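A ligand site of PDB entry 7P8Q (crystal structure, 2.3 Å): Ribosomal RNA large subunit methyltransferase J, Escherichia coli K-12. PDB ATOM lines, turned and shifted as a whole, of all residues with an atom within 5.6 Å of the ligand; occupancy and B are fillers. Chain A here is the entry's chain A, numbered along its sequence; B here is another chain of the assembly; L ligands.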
ATOM      1  N   HIS A   9     -29.724 -21.530  15.880  1.00  0.00           N
ATOM      2  CA  HIS A   9     -28.802 -21.373  17.002  1.00  0.00           C
ATOM      3  C   HIS A   9     -29.042 -20.149  17.846  1.00  0.00           C
ATOM      4  O   HIS A   9     -28.344 -19.992  18.865  1.00  0.00           O
ATOM      5  CB  HIS A   9     -27.367 -21.317  16.494  1.00  0.00           C
ATOM      6  CG  HIS A   9     -26.925 -19.984  15.965  1.00  0.00           C
ATOM      7  ND1 HIS A   9     -26.393 -18.995  16.776  1.00  0.00           N
ATOM      8  CD2 HIS A   9     -26.798 -19.543  14.695  1.00  0.00           C
ATOM      9  CE1 HIS A   9     -25.990 -17.994  16.024  1.00  0.00           C
ATOM     10  NE2 HIS A   9     -26.220 -18.289  14.758  1.00  0.00           N
ATOM     11  N   ASP A  15     -24.172 -17.908  22.102  1.00  0.00           N
ATOM     12  CA  ASP A  15     -24.788 -16.596  22.128  1.00  0.00           C
ATOM     13  C   ASP A  15     -24.824 -16.044  23.546  1.00  0.00           C
ATOM     14  O   ASP A  15     -24.269 -14.959  23.796  1.00  0.00           O
ATOM     15  CB  ASP A  15     -26.179 -16.644  21.491  1.00  0.00           C
ATOM     16  CG  ASP A  15     -26.152 -16.489  19.973  1.00  0.00           C
ATOM     17  OD1 ASP A  15     -25.059 -16.490  19.359  1.00  0.00           O
ATOM     18  OD2 ASP A  15     -27.237 -16.410  19.359  1.00  0.00           O
ATOM     19  N   LYS A  18     -21.461 -14.827  24.615  1.00  0.00           N
ATOM     20  CA  LYS A  18     -20.882 -13.693  23.912  1.00  0.00           C
ATOM     21  C   LYS A  18     -21.666 -12.427  24.197  1.00  0.00           C
ATOM     22  O   LYS A  18     -21.105 -11.380  24.506  1.00  0.00           O
ATOM     23  CB  LYS A  18     -20.785 -13.975  22.415  1.00  0.00           C
ATOM     24  CG  LYS A  18     -22.042 -13.741  21.563  1.00  0.00           C
ATOM     25  CD  LYS A  18     -21.806 -14.125  20.038  1.00  0.00           C
ATOM     26  CE  LYS A  18     -21.640 -15.628  19.840  1.00  0.00           C
ATOM     27  NZ  LYS A  18     -21.505 -16.041  18.401  1.00  0.00           N
ATOM     28  N   HIS A  19     -22.999 -12.503  24.095  1.00  0.00           N
ATOM     29  CA  HIS A  19     -23.791 -11.318  24.417  1.00  0.00           C
ATOM     30  C   HIS A  19     -23.726 -10.958  25.903  1.00  0.00           C
ATOM     31  O   HIS A  19     -24.005  -9.801  26.250  1.00  0.00           O
ATOM     32  CB  HIS A  19     -25.268 -11.469  23.999  1.00  0.00           C
ATOM     33  CG  HIS A  19     -25.436 -11.762  22.548  1.00  0.00           C
ATOM     34  ND1 HIS A  19     -26.572 -12.352  22.016  1.00  0.00           N
ATOM     35  CD2 HIS A  19     -24.591 -11.557  21.507  1.00  0.00           C
ATOM     36  CE1 HIS A  19     -26.400 -12.495  20.710  1.00  0.00           C
ATOM     37  NE2 HIS A  19     -25.195 -12.049  20.387  1.00  0.00           N
ATOM     38  N   ASP A  40     -19.264  -3.617  14.877  1.00  0.00           N
ATOM     39  CA  ASP A  40     -19.642  -5.020  14.729  1.00  0.00           C
ATOM     40  C   ASP A  40     -19.335  -5.401  13.281  1.00  0.00           C
ATOM     41  O   ASP A  40     -19.968  -4.896  12.331  1.00  0.00           O
ATOM     42  CB  ASP A  40     -21.092  -5.242  15.099  1.00  0.00           C
ATOM     43  CG  ASP A  40     -21.441  -6.725  15.235  1.00  0.00           C
ATOM     44  OD1 ASP A  40     -20.718  -7.602  14.653  1.00  0.00           O
ATOM     45  OD2 ASP A  40     -22.454  -7.014  15.915  1.00  0.00           O
ATOM     46  N   THR A  41     -18.362  -6.311  13.113  1.00  0.00           N
ATOM     47  CA  THR A  41     -17.860  -6.726  11.808  1.00  0.00           C
ATOM     48  C   THR A  41     -18.760  -7.762  11.124  1.00  0.00           C
ATOM     49  O   THR A  41     -18.896  -7.760   9.893  1.00  0.00           O
ATOM     50  CB  THR A  41     -16.467  -7.327  11.979  1.00  0.00           C
ATOM     51  OG1 THR A  41     -16.544  -8.493  12.835  1.00  0.00           O
ATOM     52  CG2 THR A  41     -15.573  -6.311  12.608  1.00  0.00           C
ATOM     53  N   HIS A  42     -19.320  -8.695  11.903  1.00  0.00           N
ATOM     54  CA  HIS A  42     -20.207  -9.738  11.369  1.00  0.00           C
ATOM     55  C   HIS A  42     -21.479  -9.622  12.182  1.00  0.00           C
ATOM     56  O   HIS A  42     -21.605 -10.366  13.159  1.00  0.00           O
ATOM     57  CB  HIS A  42     -19.626 -11.121  11.481  1.00  0.00           C
ATOM     58  CG  HIS A  42     -18.320 -11.302  10.781  1.00  0.00           C
ATOM     59  ND1 HIS A  42     -17.175 -10.639  11.152  1.00  0.00           N
ATOM     60  CD2 HIS A  42     -17.964 -12.134   9.763  1.00  0.00           C
ATOM     61  CE1 HIS A  42     -16.172 -11.039  10.392  1.00  0.00           C
ATOM     62  NE2 HIS A  42     -16.623 -11.947   9.540  1.00  0.00           N
ATOM     63  N   ALA A  43     -22.368  -8.732  11.752  1.00  0.00           N
ATOM     64  CA  ALA A  43     -23.460  -8.222  12.571  1.00  0.00           C
ATOM     65  C   ALA A  43     -24.734  -9.041  12.456  1.00  0.00           C
ATOM     66  O   ALA A  43     -25.534  -9.026  13.405  1.00  0.00           O
ATOM     67  CB  ALA A  43     -23.772  -6.778  12.167  1.00  0.00           C
ATOM     68  N   GLY A  44     -24.929  -9.782  11.337  1.00  0.00           N
ATOM     69  CA  GLY A  44     -26.205 -10.466  11.140  1.00  0.00           C
ATOM     70  C   GLY A  44     -27.417  -9.512  11.059  1.00  0.00           C
ATOM     71  O   GLY A  44     -27.306  -8.340  10.910  1.00  0.00           O
ATOM     72  N   ALA A  45     -28.609 -10.102  11.170  1.00  0.00           N
ATOM     73  CA  ALA A  45     -29.795  -9.339  10.796  1.00  0.00           C
ATOM     74  C   ALA A  45     -30.307  -8.364  11.866  1.00  0.00           C
ATOM     75  O   ALA A  45     -30.979  -7.383  11.513  1.00  0.00           O
ATOM     76  CB  ALA A  45     -30.921 -10.310  10.427  1.00  0.00           C
ATOM     77  N   TYR A  48     -34.007 -12.318  15.707  1.00  0.00           N
ATOM     78  CA  TYR A  48     -34.324 -13.620  15.156  1.00  0.00           C
ATOM     79  C   TYR A  48     -35.604 -14.149  15.768  1.00  0.00           C
ATOM     80  O   TYR A  48     -35.721 -14.331  16.981  1.00  0.00           O
ATOM     81  CB  TYR A  48     -33.159 -14.570  15.388  1.00  0.00           C
ATOM     82  CG  TYR A  48     -31.865 -14.096  14.754  1.00  0.00           C
ATOM     83  CD1 TYR A  48     -31.586 -14.336  13.413  1.00  0.00           C
ATOM     84  CD2 TYR A  48     -30.933 -13.415  15.493  1.00  0.00           C
ATOM     85  CE1 TYR A  48     -30.407 -13.929  12.836  1.00  0.00           C
ATOM     86  CE2 TYR A  48     -29.752 -13.000  14.921  1.00  0.00           C
ATOM     87  CZ  TYR A  48     -29.504 -13.248  13.589  1.00  0.00           C
ATOM     88  OH  TYR A  48     -28.337 -12.777  13.039  1.00  0.00           O
ATOM     89  N   PRO A  98     -32.503 -11.074  20.618  1.00  0.00           N
ATOM     90  CA  PRO A  98     -31.720  -9.958  20.083  1.00  0.00           C
ATOM     91  C   PRO A  98     -30.389 -10.431  19.530  1.00  0.00           C
ATOM     92  O   PRO A  98     -29.722 -11.273  20.130  1.00  0.00           O
ATOM     93  CB  PRO A  98     -31.499  -9.071  21.310  1.00  0.00           C
ATOM     94  CG  PRO A  98     -31.563 -10.015  22.417  1.00  0.00           C
ATOM     95  CD  PRO A  98     -32.684 -10.940  22.073  1.00  0.00           C
ATOM     96  N   GLY A  99     -29.966  -9.811  18.457  1.00  0.00           N
ATOM     97  CA  GLY A  99     -28.585  -9.939  18.020  1.00  0.00           C
ATOM     98  C   GLY A  99     -27.663  -8.865  18.630  1.00  0.00           C
ATOM     99  O   GLY A  99     -28.036  -7.872  19.210  1.00  0.00           O
ATOM    100  N   SER A 100     -26.378  -9.104  18.510  1.00  0.00           N
ATOM    101  CA  SER A 100     -25.418  -8.149  19.032  1.00  0.00           C
ATOM    102  C   SER A 100     -25.668  -6.707  18.583  1.00  0.00           C
ATOM    103  O   SER A 100     -25.418  -5.791  19.376  1.00  0.00           O
ATOM    104  CB  SER A 100     -24.003  -8.578  18.615  1.00  0.00           C
ATOM    105  OG  SER A 100     -23.850  -8.788  17.201  1.00  0.00           O
ATOM    106  N   PRO A 101     -26.165  -6.447  17.367  1.00  0.00           N
ATOM    107  CA  PRO A 101     -26.452  -5.045  17.019  1.00  0.00           C
ATOM    108  C   PRO A 101     -27.639  -4.474  17.777  1.00  0.00           C
ATOM    109  O   PRO A 101     -27.643  -3.285  18.147  1.00  0.00           O
ATOM    110  CB  PRO A 101     -26.701  -5.099  15.499  1.00  0.00           C
ATOM    111  CG  PRO A 101     -26.063  -6.379  15.055  1.00  0.00           C
ATOM    112  CD  PRO A 101     -26.299  -7.329  16.192  1.00  0.00           C
ATOM    113  N   THR A 117     -21.665  -3.927   9.900  1.00  0.00           N
ATOM    114  CA  THR A 117     -21.346  -4.434   8.568  1.00  0.00           C
ATOM    115  C   THR A 117     -21.861  -5.868   8.493  1.00  0.00           C
ATOM    116  O   THR A 117     -21.932  -6.590   9.499  1.00  0.00           O
ATOM    117  CB  THR A 117     -19.858  -4.283   8.332  1.00  0.00           C
ATOM    118  OG1 THR A 117     -19.447  -5.002   7.182  1.00  0.00           O
ATOM    119  CG2 THR A 117     -19.064  -4.759   9.532  1.00  0.00           C
ATOM    120  N   GLU A 118     -22.281  -6.250   7.297  1.00  0.00           N
ATOM    121  CA  GLU A 118     -23.012  -7.502   7.074  1.00  0.00           C
ATOM    122  C   GLU A 118     -23.171  -7.744   5.574  1.00  0.00           C
ATOM    123  O   GLU A 118     -24.014  -7.116   4.910  1.00  0.00           O
ATOM    124  CB  GLU A 118     -24.390  -7.464   7.737  1.00  0.00           C
ATOM    125  CG  GLU A 118     -25.299  -8.625   7.261  1.00  0.00           C
ATOM    126  CD  GLU A 118     -24.725 -10.002   7.600  1.00  0.00           C
ATOM    127  OE1 GLU A 118     -24.205 -10.191   8.717  1.00  0.00           O
ATOM    128  OE2 GLU A 118     -24.798 -10.928   6.763  1.00  0.00           O
ATOM    129  N   LEU A 119     -22.396  -8.689   5.050  1.00  0.00           N
ATOM    130  CA  LEU A 119     -22.277  -8.875   3.606  1.00  0.00           C
ATOM    131  C   LEU A 119     -23.421  -9.653   2.944  1.00  0.00           C
ATOM    132  O   LEU A 119     -23.624  -9.491   1.733  1.00  0.00           O
ATOM    133  CB  LEU A 119     -20.948  -9.588   3.348  1.00  0.00           C
ATOM    134  CG  LEU A 119     -20.375  -9.608   1.939  1.00  0.00           C
ATOM    135  CD1 LEU A 119     -20.414  -8.303   1.219  1.00  0.00           C
ATOM    136  CD2 LEU A 119     -18.956 -10.141   2.113  1.00  0.00           C
ATOM    137  N   HIS A 120     -24.184 -10.452   3.677  1.00  0.00           N
ATOM    138  CA  HIS A 120     -25.132 -11.351   2.980  1.00  0.00           C
ATOM    139  C   HIS A 120     -26.419 -10.600   2.589  1.00  0.00           C
ATOM    140  O   HIS A 120     -27.041  -9.942   3.439  1.00  0.00           O
ATOM    141  CB  HIS A 120     -25.479 -12.584   3.822  1.00  0.00           C
ATOM    142  CG  HIS A 120     -25.945 -13.772   3.023  1.00  0.00           C
ATOM    143  ND1 HIS A 120     -27.246 -13.908   2.581  1.00  0.00           N
ATOM    144  CD2 HIS A 120     -25.278 -14.849   2.564  1.00  0.00           C
ATOM    145  CE1 HIS A 120     -27.356 -15.013   1.883  1.00  0.00           C
ATOM    146  NE2 HIS A 120     -26.177 -15.612   1.860  1.00  0.00           N
ATOM    147  N   ASP A 123     -29.656 -10.673   5.019  1.00  0.00           N
ATOM    148  CA  ASP A 123     -29.789 -10.001   6.321  1.00  0.00           C
ATOM    149  C   ASP A 123     -29.597  -8.508   6.268  1.00  0.00           C
ATOM    150  O   ASP A 123     -30.204  -7.772   7.065  1.00  0.00           O
ATOM    151  CB  ASP A 123     -28.773 -10.454   7.331  1.00  0.00           C
ATOM    152  CG  ASP A 123     -28.787 -11.933   7.542  1.00  0.00           C
ATOM    153  OD1 ASP A 123     -29.844 -12.558   7.812  1.00  0.00           O
ATOM    154  OD2 ASP A 123     -27.665 -12.533   7.417  1.00  0.00           O
ATOM    155  N   ALA A 142     -20.675  -4.827   3.379  1.00  0.00           N
ATOM    156  CA  ALA A 142     -19.286  -5.002   2.979  1.00  0.00           C
ATOM    157  C   ALA A 142     -18.577  -5.996   3.893  1.00  0.00           C
ATOM    158  O   ALA A 142     -19.158  -6.529   4.840  1.00  0.00           O
ATOM    159  CB  ALA A 142     -18.525  -3.672   2.991  1.00  0.00           C
ATOM    160  N   ASP A 143     -17.295  -6.231   3.621  1.00  0.00           N
ATOM    161  CA  ASP A 143     -16.549  -7.168   4.463  1.00  0.00           C
ATOM    162  C   ASP A 143     -16.095  -6.458   5.723  1.00  0.00           C
ATOM    163  O   ASP A 143     -15.342  -5.493   5.639  1.00  0.00           O
ATOM    164  CB  ASP A 143     -15.346  -7.726   3.714  1.00  0.00           C
ATOM    165  CG  ASP A 143     -14.433  -8.505   4.627  1.00  0.00           C
ATOM    166  OD1 ASP A 143     -13.661  -7.874   5.359  1.00  0.00           O
ATOM    167  OD2 ASP A 143     -14.517  -9.752   4.606  1.00  0.00           O
ATOM    168  N   GLY A 144     -16.536  -6.969   6.888  1.00  0.00           N
ATOM    169  CA  GLY A 144     -16.274  -6.358   8.182  1.00  0.00           C
ATOM    170  C   GLY A 144     -14.820  -6.377   8.655  1.00  0.00           C
ATOM    171  O   GLY A 144     -14.444  -5.538   9.480  1.00  0.00           O
ATOM    172  N   PHE A 145     -13.986  -7.296   8.136  1.00  0.00           N
ATOM    173  CA  PHE A 145     -12.565  -7.253   8.466  1.00  0.00           C
ATOM    174  C   PHE A 145     -11.901  -5.976   7.943  1.00  0.00           C
ATOM    175  O   PHE A 145     -10.848  -5.541   8.441  1.00  0.00           O
ATOM    176  CB  PHE A 145     -11.887  -8.491   7.884  1.00  0.00           C
ATOM    177  CG  PHE A 145     -12.232  -9.775   8.605  1.00  0.00           C
ATOM    178  CD1 PHE A 145     -12.226  -9.829   9.996  1.00  0.00           C
ATOM    179  CD2 PHE A 145     -12.502 -10.925   7.892  1.00  0.00           C
ATOM    180  CE1 PHE A 145     -12.538 -11.002  10.664  1.00  0.00           C
ATOM    181  CE2 PHE A 145     -12.806 -12.127   8.574  1.00  0.00           C
ATOM    182  CZ  PHE A 145     -12.827 -12.147   9.956  1.00  0.00           C
ATOM    183  N   LEU A 162     -16.501  -5.809  18.074  1.00  0.00           N
ATOM    184  CA  LEU A 162     -17.049  -7.174  18.282  1.00  0.00           C
ATOM    185  C   LEU A 162     -16.871  -7.933  16.982  1.00  0.00           C
ATOM    186  O   LEU A 162     -17.573  -7.610  16.040  1.00  0.00           O
ATOM    187  CB  LEU A 162     -18.510  -7.145  18.732  1.00  0.00           C
ATOM    188  CG  LEU A 162     -19.097  -8.505  19.168  1.00  0.00           C
ATOM    189  CD1 LEU A 162     -19.846  -8.395  20.506  1.00  0.00           C
ATOM    190  CD2 LEU A 162     -20.010  -9.095  18.075  1.00  0.00           C
ATOM    191  N   ASP A 164     -17.196 -11.484  15.291  1.00  0.00           N
ATOM    192  CA  ASP A 164     -17.992 -12.666  15.615  1.00  0.00           C
ATOM    193  C   ASP A 164     -18.229 -13.418  14.332  1.00  0.00           C
ATOM    194  O   ASP A 164     -19.366 -13.505  13.830  1.00  0.00           O
ATOM    195  CB  ASP A 164     -19.314 -12.276  16.281  1.00  0.00           C
ATOM    196  CG  ASP A 164     -20.235 -13.483  16.499  1.00  0.00           C
ATOM    197  OD1 ASP A 164     -19.710 -14.613  16.592  1.00  0.00           O
ATOM    198  OD2 ASP A 164     -21.459 -13.304  16.578  1.00  0.00           O
ATOM    199  N   PRO A 165     -17.197 -14.016  13.782  1.00  0.00           N
ATOM    200  CA  PRO A 165     -17.304 -14.583  12.438  1.00  0.00           C
ATOM    201  C   PRO A 165     -17.963 -15.946  12.484  1.00  0.00           C
ATOM    202  O   PRO A 165     -18.050 -16.570  13.560  1.00  0.00           O
ATOM    203  CB  PRO A 165     -15.837 -14.671  11.977  1.00  0.00           C
ATOM    204  CG  PRO A 165     -15.084 -14.977  13.204  1.00  0.00           C
ATOM    205  CD  PRO A 165     -15.871 -14.259  14.362  1.00  0.00           C
ATOM    206  N   PRO A 166     -18.448 -16.440  11.341  1.00  0.00           N
ATOM    207  CA  PRO A 166     -19.101 -17.768  11.338  1.00  0.00           C
ATOM    208  C   PRO A 166     -18.131 -18.935  11.255  1.00  0.00           C
ATOM    209  O   PRO A 166     -18.538 -20.083  11.506  1.00  0.00           O
ATOM    210  CB  PRO A 166     -20.006 -17.698  10.079  1.00  0.00           C
ATOM    211  CG  PRO A 166     -19.261 -16.823   9.161  1.00  0.00           C
ATOM    212  CD  PRO A 166     -18.629 -15.749  10.050  1.00  0.00           C
ATOM    213  N   TRP A 195     -15.102 -13.710  19.283  1.00  0.00           N
ATOM    214  CA  TRP A 195     -15.738 -15.001  19.493  1.00  0.00           C
ATOM    215  C   TRP A 195     -15.019 -16.085  18.685  1.00  0.00           C
ATOM    216  O   TRP A 195     -14.589 -15.850  17.550  1.00  0.00           O
ATOM    217  CB  TRP A 195     -17.214 -14.943  19.067  1.00  0.00           C
ATOM    218  CG  TRP A 195     -17.901 -16.194  19.470  1.00  0.00           C
ATOM    219  CD1 TRP A 195     -18.141 -16.635  20.748  1.00  0.00           C
ATOM    220  CD2 TRP A 195     -18.334 -17.245  18.602  1.00  0.00           C
ATOM    221  NE1 TRP A 195     -18.719 -17.877  20.720  1.00  0.00           N
ATOM    222  CE2 TRP A 195     -18.863 -18.279  19.425  1.00  0.00           C
ATOM    223  CE3 TRP A 195     -18.353 -17.405  17.214  1.00  0.00           C
ATOM    224  CZ2 TRP A 195     -19.415 -19.441  18.902  1.00  0.00           C
ATOM    225  CZ3 TRP A 195     -18.883 -18.570  16.701  1.00  0.00           C
ATOM    226  CH2 TRP A 195     -19.412 -19.593  17.559  1.00  0.00           C
ATOM    227  P     A B   2     -22.193 -25.609  12.288  1.00  0.00           P
ATOM    228  OP1   A B   2     -22.006 -27.023  11.837  1.00  0.00           O
ATOM    229  OP2   A B   2     -22.842 -24.815  11.190  1.00  0.00           O
ATOM    230  O5'   A B   2     -23.182 -25.628  13.572  1.00  0.00           O
ATOM    231  C5'   A B   2     -22.843 -26.321  14.735  1.00  0.00           C
ATOM    232  C4'   A B   2     -23.572 -25.668  15.978  1.00  0.00           C
ATOM    233  O4'   A B   2     -22.874 -24.332  16.378  1.00  0.00           O
ATOM    234  C3'   A B   2     -24.877 -25.305  15.772  1.00  0.00           C
ATOM    235  O3'   A B   2     -25.809 -26.393  15.882  1.00  0.00           O
ATOM    236  C2'   A B   2     -25.143 -24.180  16.901  1.00  0.00           C
ATOM    237  O2'   A B   2     -25.471 -24.835  18.135  1.00  0.00           O
ATOM    238  C1'   A B   2     -24.009 -23.406  16.908  1.00  0.00           C
ATOM    239  N9    A B   2     -23.519 -22.309  15.996  1.00  0.00           N
ATOM    240  C8    A B   2     -23.253 -22.354  14.688  1.00  0.00           C
ATOM    241  N7    A B   2     -22.837 -21.153  14.299  1.00  0.00           N
ATOM    242  C5    A B   2     -22.839 -20.332  15.353  1.00  0.00           C
ATOM    243  C6    A B   2     -22.517 -18.989  15.585  1.00  0.00           C
ATOM    244  N6    A B   2     -22.023 -18.110  14.490  1.00  0.00           N
ATOM    245  N1    A B   2     -22.648 -18.502  16.798  1.00  0.00           N
ATOM    246  C2    A B   2     -23.067 -19.238  17.812  1.00  0.00           C
ATOM    247  N3    A B   2     -23.373 -20.500  17.622  1.00  0.00           N
ATOM    248  C4    A B   2     -23.276 -21.072  16.431  1.00  0.00           C
HETATM  249  C1  LIG L   1     -21.272 -16.886  14.819  1.00  0.00           C
HETATM  250  C2  LIG L   1     -21.531 -15.752  13.773  1.00  0.00           C
HETATM  251  C3  LIG L   1     -22.984 -15.758  13.148  1.00  0.00           C
HETATM  252  C4  LIG L   1     -23.299 -13.248  13.181  1.00  0.00           C
HETATM  253  C5  LIG L   1     -24.653 -11.947  15.005  1.00  0.00           C
HETATM  254  C6  LIG L   1     -22.270 -14.370  11.200  1.00  0.00           C
HETATM  255  C7  LIG L   1     -23.758 -14.015   9.052  1.00  0.00           C
HETATM  256  C8  LIG L   1     -20.079 -13.706   6.807  1.00  0.00           C
HETATM  257  C9  LIG L   1     -18.992 -11.868   6.546  1.00  0.00           C
HETATM  258  N1  LIG L   1     -23.232 -14.510  12.354  1.00  0.00           N
HETATM  259  C10 LIG L   1     -24.199 -13.366  14.442  1.00  0.00           C
HETATM  260  N2  LIG L   1     -23.507 -11.034  14.985  1.00  0.00           N
HETATM  261  C11 LIG L   1     -25.149 -12.090  16.443  1.00  0.00           C
HETATM  262  O1  LIG L   1     -26.226 -12.675  16.722  1.00  0.00           O
HETATM  263  O2  LIG L   1     -24.426 -11.626  17.338  1.00  0.00           O
HETATM  264  C12 LIG L   1     -22.808 -13.332  10.129  1.00  0.00           C
HETATM  265  O3  LIG L   1     -21.822 -12.824   9.491  1.00  0.00           O
HETATM  266  C13 LIG L   1     -22.163 -12.816   7.924  1.00  0.00           C
HETATM  267  C14 LIG L   1     -22.950 -13.917   7.728  1.00  0.00           C
HETATM  268  O4  LIG L   1     -23.822 -13.830   6.598  1.00  0.00           O
HETATM  269  O5  LIG L   1     -25.024 -13.397   8.913  1.00  0.00           O
HETATM  270  N3  LIG L   1     -20.834 -12.743   7.267  1.00  0.00           N
HETATM  271  N4  LIG L   1     -18.953 -13.187   6.352  1.00  0.00           N
HETATM  272  C15 LIG L   1     -18.126 -10.797   6.308  1.00  0.00           C
HETATM  273  N5  LIG L   1     -16.840 -11.047   5.669  1.00  0.00           N
HETATM  274  N6  LIG L   1     -18.508  -9.578   6.647  1.00  0.00           N
HETATM  275  C16 LIG L   1     -19.664  -9.345   7.224  1.00  0.00           C
HETATM  276  N7  LIG L   1     -20.495 -10.326   7.484  1.00  0.00           N
HETATM  277  C17 LIG L   1     -20.181 -11.581   7.157  1.00  0.00           C
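Lys 18 touches the ligand.
O of Thr 41 touches C16 of the ligand (3.2 Å).
CA of Gly 44 touches O5 of the ligand, 3.9 Å away.
CE2 of Tyr 48 touches O1 of the ligand, at 3.97 Å.
Gly 99 touches the ligand (CA to O1, 3.8 Å).
CB of His 120 touches O4 of the ligand, at 3.5 Å.
Ala 142 touches the ligand (O to N6, 3.6 Å).
Pro 165 touches the ligand (O to C1, 3.5 Å).
Pro 166 touches the ligand.
CZ3 of Trp 195 touches C1 of the ligand (3.5 Å).
Hydrophobic or aromatic side chains that line the ligand: His 19, His 42, Tyr 48, His 120, Pro 166 and Trp 195.
21 residues have an atom within 4 Å of the ligand: Lys 18, His 19, Thr 41, His 42, Ala 43, Gly 44, Tyr 48, Gly 99, Ser 100, Glu 118, Leu 119, His 120, Asp 123, Ala 142, Asp 143, Gly 144, Asp 164, Pro 165, Pro 166, Trp 195 and A 2 of chain B.
The nearest printed residue that does not touch the ligand is Thr 117 (4.2 Å).
The backbone carbonyl oxygen (O) of Thr 117 is in hydrogen-bond range of the backbone NH (N) of Ala 43.
The backbone NH (N) of Thr 41 sits at hydrogen-bond distance from the backbone carbonyl oxygen (O) of Leu 162, at 3.3 Å.
The side-chain hydroxyl (OG) of Ser 100 is in hydrogen-bond range of the side-chain carboxylate (OD2) of Asp 40.
The backbone NH of Gly 44 is in hydrogen-bond range of the side-chain carboxylate of Glu 118, at 2.7 Å.
The side-chain carboxylate of Asp 15 lies within salt-bridge range of the side-chain amino group of Lys 18, 3.7 Å away.
The backbone NH (N) of Ala 45 lies within hydrogen-bond range of the side-chain hydroxyl (OH) of Tyr 48 (3.3 Å).
N1 of A 2 of chain B lies within hydrogen-bond range of NZ of Lys 18 (3.2 Å).
The backbone carbonyl oxygen of Ala 142 lies within hydrogen-bond range of the side-chain hydroxyl of Thr 117, at 2.8 Å.
The backbone NH of Leu 119 lies within hydrogen-bond range of a nitrogen (N7) of the ligand, at 3.5 Å.
The side-chain carboxylate (OD2) of Asp 123 lies within hydrogen-bond range of an oxygen (O5) of the ligand, 3.2 Å away.
A nitrogen (N6) of the ligand sits at hydrogen-bond distance from the backbone NH of Gly 144, 3.3 Å away.
The side-chain carboxylate (OD2) of Asp 164 is in salt-bridge range of a nitrogen (N2) of the ligand, at 3.4 Å.
O2 of the ligand lies within hydrogen-bond range of NE2 of His 19 (3.2 Å).
O2 of the ligand sits at hydrogen-bond distance from OG of Ser 100 (2.9 Å).
N5 of the ligand sits at hydrogen-bond distance from OD2 of Asp 143 (2.9 Å).
The side-chain carboxylate (OE2) of Glu 118 is in hydrogen-bond range of an oxygen (O4) of the ligand, at 3.1 Å.
N6 of A 2 of chain B is bonded to a carbon (C1) of the ligand (1.5 Å).
N2 of the ligand lies within hydrogen-bond range of O of His 42.
The backbone NH of Ser 100 sits close to an oxygen (O2) of the ligand, at 3.4 Å.
The backbone carbonyl oxygen (O) of Ala 43 sits at hydrogen-bond distance from a nitrogen (N2) of the ligand.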
